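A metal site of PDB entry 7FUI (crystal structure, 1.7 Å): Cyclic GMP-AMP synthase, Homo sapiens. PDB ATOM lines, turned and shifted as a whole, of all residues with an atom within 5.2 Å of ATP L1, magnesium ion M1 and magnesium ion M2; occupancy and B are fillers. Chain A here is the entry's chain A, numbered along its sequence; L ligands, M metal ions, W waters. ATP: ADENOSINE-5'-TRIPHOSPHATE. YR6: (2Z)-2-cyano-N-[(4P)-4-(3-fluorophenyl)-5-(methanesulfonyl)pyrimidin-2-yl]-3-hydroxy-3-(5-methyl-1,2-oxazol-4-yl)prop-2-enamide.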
ATOM      1  N   GLY A  52     -28.995 -14.106  30.870  1.00  0.00           N
ATOM      2  CA  GLY A  52     -28.033 -14.894  30.087  1.00  0.00           C
ATOM      3  C   GLY A  52     -28.089 -16.376  30.415  1.00  0.00           C
ATOM      4  O   GLY A  52     -28.991 -16.810  31.165  1.00  0.00           O
ATOM      5  N   SER A  53     -27.151 -17.134  29.861  1.00  0.00           N
ATOM      6  CA  SER A  53     -27.270 -18.597  29.665  1.00  0.00           C
ATOM      7  C   SER A  53     -27.253 -19.330  31.013  1.00  0.00           C
ATOM      8  O   SER A  53     -27.891 -20.372  31.142  1.00  0.00           O
ATOM      9  CB  SER A  53     -26.179 -19.090  28.750  1.00  0.00           C
ATOM     10  OG  SER A  53     -24.903 -18.830  29.305  1.00  0.00           O
ATOM     11  N   TYR A  54     -26.581 -18.780  32.017  1.00  0.00           N
ATOM     12  CA  TYR A  54     -26.529 -19.502  33.315  1.00  0.00           C
ATOM     13  C   TYR A  54     -27.929 -19.597  33.920  1.00  0.00           C
ATOM     14  O   TYR A  54     -28.338 -20.672  34.361  1.00  0.00           O
ATOM     15  CB  TYR A  54     -25.628 -18.766  34.284  1.00  0.00           C
ATOM     16  CG  TYR A  54     -25.560 -19.483  35.607  1.00  0.00           C
ATOM     17  CD1 TYR A  54     -24.748 -20.593  35.791  1.00  0.00           C
ATOM     18  CD2 TYR A  54     -26.385 -19.077  36.639  1.00  0.00           C
ATOM     19  CE1 TYR A  54     -24.705 -21.243  37.018  1.00  0.00           C
ATOM     20  CE2 TYR A  54     -26.369 -19.739  37.856  1.00  0.00           C
ATOM     21  CZ  TYR A  54     -25.533 -20.820  38.044  1.00  0.00           C
ATOM     22  OH  TYR A  54     -25.553 -21.417  39.284  1.00  0.00           O
ATOM     23  N   GLU A  56     -30.776 -19.188  32.418  1.00  0.00           N
ATOM     24  CA  GLU A  56     -31.650 -19.811  31.394  1.00  0.00           C
ATOM     25  C   GLU A  56     -31.394 -21.323  31.350  1.00  0.00           C
ATOM     26  O   GLU A  56     -32.141 -22.032  30.627  1.00  0.00           O
ATOM     27  CB  GLU A  56     -31.421 -19.169  30.024  1.00  0.00           C
ATOM     28  CG  GLU A  56     -31.718 -17.696  29.973  1.00  0.00           C
ATOM     29  CD  GLU A  56     -31.240 -16.985  28.710  1.00  0.00           C
ATOM     30  OE1 GLU A  56     -30.245 -17.455  28.079  1.00  0.00           O
ATOM     31  OE2 GLU A  56     -31.926 -15.999  28.313  1.00  0.00           O
ATOM     32  N   LYS A  59     -26.253 -22.585  29.737  1.00  0.00           N
ATOM     33  CA  LYS A  59     -24.763 -22.487  29.860  1.00  0.00           C
ATOM     34  C   LYS A  59     -24.162 -23.873  29.642  1.00  0.00           C
ATOM     35  O   LYS A  59     -24.695 -24.838  30.240  1.00  0.00           O
ATOM     36  CB  LYS A  59     -24.372 -21.965  31.239  1.00  0.00           C
ATOM     37  CG  LYS A  59     -22.873 -21.755  31.448  1.00  0.00           C
ATOM     38  CD  LYS A  59     -22.364 -20.476  30.838  1.00  0.00           C
ATOM     39  CE  LYS A  59     -20.839 -20.368  30.758  1.00  0.00           C
ATOM     40  NZ  LYS A  59     -20.238 -21.431  29.914  1.00  0.00           N
ATOM     41  N   GLU A  65     -19.168 -18.153  33.285  1.00  0.00           N
ATOM     42  CA  GLU A  65     -19.608 -16.854  32.683  1.00  0.00           C
ATOM     43  C   GLU A  65     -21.065 -16.608  33.053  1.00  0.00           C
ATOM     44  O   GLU A  65     -21.956 -17.463  32.691  1.00  0.00           O
ATOM     45  CB  GLU A  65     -19.384 -16.816  31.164  1.00  0.00           C
ATOM     46  CG  GLU A  65     -19.211 -15.401  30.596  1.00  0.00           C
ATOM     47  CD  GLU A  65     -20.503 -14.736  30.144  1.00  0.00           C
ATOM     48  OE1 GLU A  65     -21.536 -15.447  30.122  1.00  0.00           O
ATOM     49  OE2 GLU A  65     -20.462 -13.531  29.823  1.00  0.00           O
ATOM     50  N   PHE A  66     -21.271 -15.555  33.826  1.00  0.00           N
ATOM     51  CA  PHE A  66     -22.565 -15.075  34.397  1.00  0.00           C
ATOM     52  C   PHE A  66     -22.833 -13.659  33.854  1.00  0.00           C
ATOM     53  O   PHE A  66     -21.890 -12.864  33.661  1.00  0.00           O
ATOM     54  CB  PHE A  66     -22.484 -15.011  35.909  1.00  0.00           C
ATOM     55  CG  PHE A  66     -22.372 -16.340  36.603  1.00  0.00           C
ATOM     56  CD1 PHE A  66     -21.199 -17.068  36.546  1.00  0.00           C
ATOM     57  CD2 PHE A  66     -23.432 -16.857  37.331  1.00  0.00           C
ATOM     58  CE1 PHE A  66     -21.098 -18.289  37.185  1.00  0.00           C
ATOM     59  CE2 PHE A  66     -23.318 -18.068  38.008  1.00  0.00           C
ATOM     60  CZ  PHE A  66     -22.136 -18.764  37.936  1.00  0.00           C
ATOM     61  N   ASP A  67     -24.095 -13.316  33.731  1.00  0.00           N
ATOM     62  CA  ASP A  67     -24.562 -12.019  33.200  1.00  0.00           C
ATOM     63  C   ASP A  67     -25.568 -11.455  34.163  1.00  0.00           C
ATOM     64  O   ASP A  67     -26.473 -12.204  34.593  1.00  0.00           O
ATOM     65  CB  ASP A  67     -25.127 -12.166  31.787  1.00  0.00           C
ATOM     66  CG  ASP A  67     -24.135 -12.791  30.849  1.00  0.00           C
ATOM     67  OD1 ASP A  67     -23.252 -12.047  30.378  1.00  0.00           O
ATOM     68  OD2 ASP A  67     -24.263 -14.023  30.559  1.00  0.00           O
ATOM     69  N   ASP A 159     -20.326 -10.450  33.637  1.00  0.00           N
ATOM     70  CA  ASP A 159     -20.657  -9.242  32.852  1.00  0.00           C
ATOM     71  C   ASP A 159     -21.775  -8.541  33.600  1.00  0.00           C
ATOM     72  O   ASP A 159     -22.803  -9.187  33.892  1.00  0.00           O
ATOM     73  CB  ASP A 159     -21.092  -9.557  31.409  1.00  0.00           C
ATOM     74  CG  ASP A 159     -20.030 -10.104  30.476  1.00  0.00           C
ATOM     75  OD1 ASP A 159     -18.837  -9.840  30.729  1.00  0.00           O
ATOM     76  OD2 ASP A 159     -20.422 -10.824  29.506  1.00  0.00           O
ATOM     77  N   ARG A 216     -28.921   1.014  23.397  1.00  0.00           N
ATOM     78  CA  ARG A 216     -29.588  -0.009  22.569  1.00  0.00           C
ATOM     79  C   ARG A 216     -30.662  -0.748  23.369  1.00  0.00           C
ATOM     80  O   ARG A 216     -30.422  -1.031  24.553  1.00  0.00           O
ATOM     81  CB  ARG A 216     -28.558  -0.986  22.025  1.00  0.00           C
ATOM     82  CG  ARG A 216     -29.068  -1.789  20.829  1.00  0.00           C
ATOM     83  CD  ARG A 216     -28.468  -3.169  20.715  1.00  0.00           C
ATOM     84  NE  ARG A 216     -28.895  -3.918  21.889  1.00  0.00           N
ATOM     85  CZ  ARG A 216     -28.127  -4.657  22.685  1.00  0.00           C
ATOM     86  NH1 ARG A 216     -28.664  -5.180  23.751  1.00  0.00           N
ATOM     87  NH2 ARG A 216     -26.833  -4.863  22.426  1.00  0.00           N
ATOM     88  N   LEU A 217     -31.779  -1.103  22.737  1.00  0.00           N
ATOM     89  CA  LEU A 217     -32.823  -1.906  23.436  1.00  0.00           C
ATOM     90  C   LEU A 217     -32.250  -3.250  23.907  1.00  0.00           C
ATOM     91  O   LEU A 217     -31.384  -3.852  23.208  1.00  0.00           O
ATOM     92  CB  LEU A 217     -34.015  -2.127  22.520  1.00  0.00           C
ATOM     93  CG  LEU A 217     -34.827  -0.873  22.203  1.00  0.00           C
ATOM     94  CD1 LEU A 217     -35.887  -1.211  21.158  1.00  0.00           C
ATOM     95  CD2 LEU A 217     -35.474  -0.354  23.488  1.00  0.00           C
ATOM     96  N   SER A 220     -33.392  -8.945  27.437  1.00  0.00           N
ATOM     97  CA  SER A 220     -32.755 -10.116  28.107  1.00  0.00           C
ATOM     98  C   SER A 220     -33.699 -10.747  29.129  1.00  0.00           C
ATOM     99  O   SER A 220     -33.708 -11.985  29.262  1.00  0.00           O
ATOM    100  CB  SER A 220     -31.461  -9.723  28.751  1.00  0.00           C
ATOM    101  OG  SER A 220     -30.601  -9.185  27.773  1.00  0.00           O
ATOM    102  N   GLU A 223     -36.219 -12.823  27.209  1.00  0.00           N
ATOM    103  CA  GLU A 223     -35.518 -14.021  26.676  1.00  0.00           C
ATOM    104  C   GLU A 223     -35.471 -15.074  27.795  1.00  0.00           C
ATOM    105  O   GLU A 223     -35.705 -16.270  27.523  1.00  0.00           O
ATOM    106  CB  GLU A 223     -34.119 -13.675  26.170  1.00  0.00           C
ATOM    107  CG  GLU A 223     -34.088 -12.712  25.014  1.00  0.00           C
ATOM    108  CD  GLU A 223     -32.723 -12.188  24.600  1.00  0.00           C
ATOM    109  OE1 GLU A 223     -31.704 -12.714  25.082  1.00  0.00           O
ATOM    110  OE2 GLU A 223     -32.676 -11.254  23.770  1.00  0.00           O
ATOM    111  N   LYS A 254     -24.844 -23.913  20.419  1.00  0.00           N
ATOM    112  CA  LYS A 254     -23.850 -23.038  21.094  1.00  0.00           C
ATOM    113  C   LYS A 254     -22.479 -23.718  21.004  1.00  0.00           C
ATOM    114  O   LYS A 254     -21.500 -23.027  20.679  1.00  0.00           O
ATOM    115  CB  LYS A 254     -24.237 -22.804  22.546  1.00  0.00           C
ATOM    116  CG  LYS A 254     -25.440 -21.896  22.749  1.00  0.00           C
ATOM    117  CD  LYS A 254     -26.033 -22.008  24.135  1.00  0.00           C
ATOM    118  CE  LYS A 254     -25.207 -21.374  25.236  1.00  0.00           C
ATOM    119  NZ  LYS A 254     -24.724 -20.015  24.891  1.00  0.00           N
ATOM    120  N   GLU A 258     -19.029 -22.501  19.399  1.00  0.00           N
ATOM    121  CA  GLU A 258     -17.830 -22.351  20.272  1.00  0.00           C
ATOM    122  C   GLU A 258     -16.681 -23.179  19.658  1.00  0.00           C
ATOM    123  O   GLU A 258     -15.542 -22.695  19.582  1.00  0.00           O
ATOM    124  CB  GLU A 258     -18.107 -22.787  21.715  1.00  0.00           C
ATOM    125  CG  GLU A 258     -19.039 -21.872  22.514  1.00  0.00           C
ATOM    126  CD  GLU A 258     -19.201 -22.197  24.006  1.00  0.00           C
ATOM    127  OE1 GLU A 258     -18.440 -23.096  24.466  1.00  0.00           O
ATOM    128  OE2 GLU A 258     -20.060 -21.525  24.743  1.00  0.00           O
ATOM    129  N   SER A 275     -22.594 -16.234  20.445  1.00  0.00           N
ATOM    130  CA  SER A 275     -23.651 -17.153  20.913  1.00  0.00           C
ATOM    131  C   SER A 275     -25.024 -16.501  20.723  1.00  0.00           C
ATOM    132  O   SER A 275     -25.989 -17.254  20.531  1.00  0.00           O
ATOM    133  CB  SER A 275     -23.399 -17.586  22.348  1.00  0.00           C
ATOM    134  OG  SER A 275     -23.630 -16.520  23.264  1.00  0.00           O
ATOM    135  N   TYR A 276     -25.124 -15.166  20.724  1.00  0.00           N
ATOM    136  CA  TYR A 276     -26.428 -14.463  20.600  1.00  0.00           C
ATOM    137  C   TYR A 276     -26.992 -14.647  19.169  1.00  0.00           C
ATOM    138  O   TYR A 276     -28.239 -14.635  19.031  1.00  0.00           O
ATOM    139  CB  TYR A 276     -26.339 -12.964  20.922  1.00  0.00           C
ATOM    140  CG  TYR A 276     -27.703 -12.300  21.034  1.00  0.00           C
ATOM    141  CD1 TYR A 276     -28.597 -12.679  22.019  1.00  0.00           C
ATOM    142  CD2 TYR A 276     -28.139 -11.339  20.128  1.00  0.00           C
ATOM    143  CE1 TYR A 276     -29.828 -12.067  22.148  1.00  0.00           C
ATOM    144  CE2 TYR A 276     -29.406 -10.757  20.221  1.00  0.00           C
ATOM    145  CZ  TYR A 276     -30.262 -11.135  21.229  1.00  0.00           C
ATOM    146  OH  TYR A 276     -31.505 -10.576  21.388  1.00  0.00           O
ATOM    147  N   LYS A 279     -28.630 -17.995  19.538  1.00  0.00           N
ATOM    148  CA  LYS A 279     -29.816 -17.899  20.429  1.00  0.00           C
ATOM    149  C   LYS A 279     -30.992 -17.303  19.645  1.00  0.00           C
ATOM    150  O   LYS A 279     -32.095 -17.844  19.741  1.00  0.00           O
ATOM    151  CB  LYS A 279     -29.460 -17.082  21.678  1.00  0.00           C
ATOM    152  CG  LYS A 279     -30.530 -17.042  22.751  1.00  0.00           C
ATOM    153  CD  LYS A 279     -30.272 -15.981  23.820  1.00  0.00           C
ATOM    154  CE  LYS A 279     -31.051 -16.168  25.108  1.00  0.00           C
ATOM    155  NZ  LYS A 279     -30.909 -15.017  26.039  1.00  0.00           N
ATOM    156  N   ASN A 322     -33.253  -9.641  14.675  1.00  0.00           N
ATOM    157  CA  ASN A 322     -33.438  -9.566  16.133  1.00  0.00           C
ATOM    158  C   ASN A 322     -34.859 -10.053  16.431  1.00  0.00           C
ATOM    159  O   ASN A 322     -35.822  -9.700  15.707  1.00  0.00           O
ATOM    160  CB  ASN A 322     -33.100  -8.164  16.633  1.00  0.00           C
ATOM    161  CG  ASN A 322     -33.303  -7.983  18.120  1.00  0.00           C
ATOM    162  OD1 ASN A 322     -34.427  -8.121  18.616  1.00  0.00           O
ATOM    163  ND2 ASN A 322     -32.231  -7.670  18.819  1.00  0.00           N
HETATM  164  PG  ATP L   1     -23.085 -17.585  26.743  1.00  0.00           P
HETATM  165  O1G ATP L   1     -22.667 -16.578  27.782  1.00  0.00           O
HETATM  166  O2G ATP L   1     -22.309 -17.480  25.451  1.00  0.00           O
HETATM  167  O3G ATP L   1     -23.210 -18.977  27.276  1.00  0.00           O
HETATM  168  PB  ATP L   1     -25.310 -15.791  26.829  1.00  0.00           P
HETATM  169  O1B ATP L   1     -26.690 -15.760  26.290  1.00  0.00           O
HETATM  170  O2B ATP L   1     -25.125 -15.601  28.313  1.00  0.00           O
HETATM  171  O3B ATP L   1     -24.588 -17.133  26.402  1.00  0.00           O
HETATM  172  PA  ATP L   1     -23.690 -13.356  26.557  1.00  0.00           P
HETATM  173  O1A ATP L   1     -22.808 -12.947  25.453  1.00  0.00           O
HETATM  174  O2A ATP L   1     -23.087 -13.594  27.919  1.00  0.00           O
HETATM  175  O3A ATP L   1     -24.410 -14.695  26.098  1.00  0.00           O
HETATM  176  O5' ATP L   1     -24.917 -12.320  26.643  1.00  0.00           O
HETATM  177  C5' ATP L   1     -25.779 -12.221  27.794  1.00  0.00           C
HETATM  178  C4' ATP L   1     -27.137 -11.773  27.310  1.00  0.00           C
HETATM  179  O4' ATP L   1     -26.999 -10.452  26.750  1.00  0.00           O
HETATM  180  C3' ATP L   1     -27.787 -12.574  26.182  1.00  0.00           C
HETATM  181  O3' ATP L   1     -28.399 -13.784  26.625  1.00  0.00           O
HETATM  182  C2' ATP L   1     -28.757 -11.523  25.632  1.00  0.00           C
HETATM  183  O2' ATP L   1     -29.923 -11.359  26.429  1.00  0.00           O
HETATM  184  C1' ATP L   1     -27.897 -10.259  25.683  1.00  0.00           C
HETATM  185  N9  ATP L   1     -27.143  -9.981  24.450  1.00  0.00           N
HETATM  186  C8  ATP L   1     -25.892 -10.406  24.095  1.00  0.00           C
HETATM  187  N7  ATP L   1     -25.523  -9.988  22.914  1.00  0.00           N
HETATM  188  C5  ATP L   1     -26.592  -9.224  22.455  1.00  0.00           C
HETATM  189  C6  ATP L   1     -26.821  -8.508  21.250  1.00  0.00           C
HETATM  190  N6  ATP L   1     -25.954  -8.432  20.239  1.00  0.00           N
HETATM  191  N1  ATP L   1     -28.019  -7.891  21.110  1.00  0.00           N
HETATM  192  C2  ATP L   1     -28.897  -7.972  22.112  1.00  0.00           C
HETATM  193  N3  ATP L   1     -28.778  -8.590  23.298  1.00  0.00           N
HETATM  194  C4  ATP L   1     -27.591  -9.220  23.388  1.00  0.00           C
HETATM  195  C10 YR6 L   2     -22.300  -7.305  21.932  1.00  0.00           C
HETATM  196  O14 YR6 L   2     -20.147  -6.574  20.637  1.00  0.00           O
HETATM  197  C15 YR6 L   2     -21.839  -8.010  23.092  1.00  0.00           C
HETATM  198  C16 YR6 L   2     -20.588  -8.810  23.237  1.00  0.00           C
HETATM  199  C17 YR6 L   2     -19.317  -8.284  23.046  1.00  0.00           C
HETATM  200  C18 YR6 L   2     -18.180  -9.080  23.188  1.00  0.00           C
HETATM  201  C19 YR6 L   2     -18.296 -10.424  23.509  1.00  0.00           C
HETATM  202  C20 YR6 L   2     -19.568 -10.925  23.699  1.00  0.00           C
HETATM  203  C21 YR6 L   2     -20.712 -10.166  23.561  1.00  0.00           C
HETATM  204  C24 YR6 L   2     -25.655  -8.009  27.848  1.00  0.00           C
HETATM  205  C26 YR6 L   2     -26.277  -8.303  29.115  1.00  0.00           C
HETATM  206  C27 YR6 L   2     -25.706  -8.582  30.323  1.00  0.00           C
HETATM  207  N1  YR6 L   2     -28.661  -6.296  27.335  1.00  0.00           N
HETATM  208  C2  YR6 L   2     -27.604  -6.725  27.153  1.00  0.00           C
HETATM  209  C3  YR6 L   2     -26.309  -7.275  26.865  1.00  0.00           C
HETATM  210  C4  YR6 L   2     -25.739  -7.003  25.556  1.00  0.00           C
HETATM  211  O5  YR6 L   2     -26.375  -6.347  24.709  1.00  0.00           O
HETATM  212  N6  YR6 L   2     -24.505  -7.515  25.326  1.00  0.00           N
HETATM  213  C7  YR6 L   2     -23.817  -7.460  24.146  1.00  0.00           C
HETATM  214  N8  YR6 L   2     -24.312  -6.727  23.144  1.00  0.00           N
HETATM  215  C9  YR6 L   2     -23.538  -6.678  22.039  1.00  0.00           C
HETATM  216  S11 YR6 L   2     -21.404  -7.210  20.403  1.00  0.00           S
HETATM  217  C12 YR6 L   2     -21.109  -8.876  19.939  1.00  0.00           C
HETATM  218  O13 YR6 L   2     -22.294  -6.623  19.433  1.00  0.00           O
HETATM  219  F22 YR6 L   2     -19.718 -12.256  24.032  1.00  0.00           F
HETATM  220  N23 YR6 L   2     -22.639  -8.092  24.165  1.00  0.00           N
HETATM  221  O25 YR6 L   2     -24.422  -8.521  27.618  1.00  0.00           O
HETATM  222  O28 YR6 L   2     -26.668  -8.877  31.220  1.00  0.00           O
HETATM  223  N29 YR6 L   2     -27.920  -8.871  30.557  1.00  0.00           N
HETATM  224  C30 YR6 L   2     -27.646  -8.576  29.321  1.00  0.00           C
HETATM  225  C31 YR6 L   2     -24.321  -8.535  30.852  1.00  0.00           C
HETATM  226 MG    MG M   1     -21.817 -12.206  28.961  1.00  0.00          MG
HETATM  227 MG    MG M   2     -23.384 -15.279  29.230  1.00  0.00          MG
HETATM  228  O   HOH W   1     -26.440 -16.020  23.552  1.00  0.00           O
HETATM  229  O   HOH W   2     -20.494 -12.317  27.183  1.00  0.00           O
HETATM  230  O   HOH W   3     -20.624 -15.593  24.823  1.00  0.00           O
HETATM  231  O   HOH W   4     -23.341 -13.544  22.773  1.00  0.00           O
HETATM  232  O   HOH W   5     -29.344  -7.325  18.879  1.00  0.00           O
HETATM  233  O   HOH W   6     -21.937 -21.342  27.527  1.00  0.00           O
HETATM  234  O   HOH W   7     -28.445 -17.904  26.320  1.00  0.00           O
HETATM  235  O   HOH W   8     -22.185 -20.300  23.633  1.00  0.00           O
HETATM  236  O   HOH W   9     -23.407 -10.573  21.292  1.00  0.00           O
HETATM  237  O   HOH W  10     -19.837 -16.886  27.867  1.00  0.00           O
HETATM  238  O   HOH W  11     -23.896 -16.863  30.651  1.00  0.00           O
HETATM  239  O   HOH W  12     -22.676 -10.514  27.945  1.00  0.00           O
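Magnesium ion M1 is bound by OD1 of Asp 67 (2.0 Å), OD2 of Asp 159 (2.0 Å), OE2 of Glu 65 (2.1 Å), O2A of ATP L1 (2.2 Å), water W12 (2.2 Å) and water W2 (2.2 Å).
Magnesium ion M1 has six donor atoms within binding distance.
Within 4 Å of magnesium ion M1: Glu 65, Asp 67 and Asp 159.
The nearest printed residue that does not touch magnesium ion M1 is Phe 66 (4.7 Å).
Gly 52 touches ATP L1 (CA to O2B, 3.5 Å).
CD of Lys 59 touches O3G of ATP L1 (3.96 Å).
CE2 of Tyr 276 touches N1 of ATP L1, 3.3 Å away.
Hydrophobic or aromatic side chains that line ATP L1: Tyr 276.
Along chain A the residues within 4 Å of ATP L1 span positions 52 to 279.
The nearest printed residue that does not touch ATP L1 is Asp 159 (4.2 Å).
Ser 53 touches magnesium ion M2.
Within 4 Å of magnesium ion M2: Ser 53, Glu 65 and Asp 67.
The nearest printed residue that does not touch magnesium ion M2 is Gly 52 (4.7 Å).
OG of Ser 275 is in hydrogen-bond range of O2G of ATP L1.
The guanidinium group of Arg 216 is in hydrogen-bond range of an oxygen (O5) of YR6 L2, at 2.7 Å.
O3' of ATP L1 is in hydrogen-bond range of NZ of Lys 279 (2.9 Å).
O3G of ATP L1 lies within hydrogen-bond range of OG of Ser 53 (2.6 Å).
The backbone NH of Ser 53 sits close to an oxygen (O2B) of ATP L1 (3.0 Å).
An oxygen (O2') of ATP L1 sits at hydrogen-bond distance from the side-chain hydroxyl of Ser 220.
An oxygen (O3G) of ATP L1 lies within salt-bridge range of the side-chain amino group (NZ) of Lys 254 (3.0 Å).
O2' of ATP L1 sits at hydrogen-bond distance from OE1 of Glu 223 (2.6 Å).
A nitrogen (N3) of ATP L1 lies close to the guanidinium group of Arg 216 (3.4 Å).
Water W12 lies within hydrogen-bond range of O25 of YR6 L2 (2.7 Å) and O5' of ATP L1 (3.2 Å).
Water W11 bridges OG of Ser 53 (2.6 Å) and O of Glu 65 (2.9 Å).
Water W5 bridges N1 of ATP L1 and ND2 of Asn 322.
Water W7 lies within hydrogen-bond range of the side-chain carboxylate (OE1) of Glu 56 and an oxygen (O1B) of ATP L1.
Water W4 lies within hydrogen-bond range of O1A of ATP L1 (2.8 Å), OG of Ser 275 (3.0 Å) and N of Tyr 276 (3.2 Å).
Water W8 lies within hydrogen-bond range of the side-chain carboxylate of Glu 258 (2.7 Å), the side-chain amino group of Lys 254 (2.8 Å) and an oxygen (O2G) of ATP L1 (3.4 Å).
An oxygen (O4') of ATP L1 lies close to an oxygen (O25) of YR6 L2 (3.3 Å).
Magnesium ion M2 is bound by O2B of ATP L1 (2.0 Å).
The side-chain carboxylate (OD2) of Asp 67 is bound to magnesium ion M2, at 2.0 Å.
OE1 of Glu 65 binds magnesium ion M2.
O1G of ATP L1 is bound to magnesium ion M2 (2.1 Å).
O2A of ATP L1 binds magnesium ion M2, 2.2 Å away.
Magnesium ion M2 is bound by water W11, 2.2 Å away.
NZ of Lys 279 is in salt-bridge range of OE2 of Glu 56, at 2.7 Å.
The backbone carbonyl oxygen (O) of Ser 53 sits at hydrogen-bond distance from the backbone NH (N) of Lys 59 (3.1 Å).
NZ of Lys 279 is in salt-bridge range of OE1 of Glu 223 (2.6 Å).
The side-chain carboxylate of Glu 223 lies within hydrogen-bond range of the side-chain hydroxyl of Tyr 276 (2.7 Å).
O of Phe 66 is in hydrogen-bond range of N of Asp 159, at 2.9 Å.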
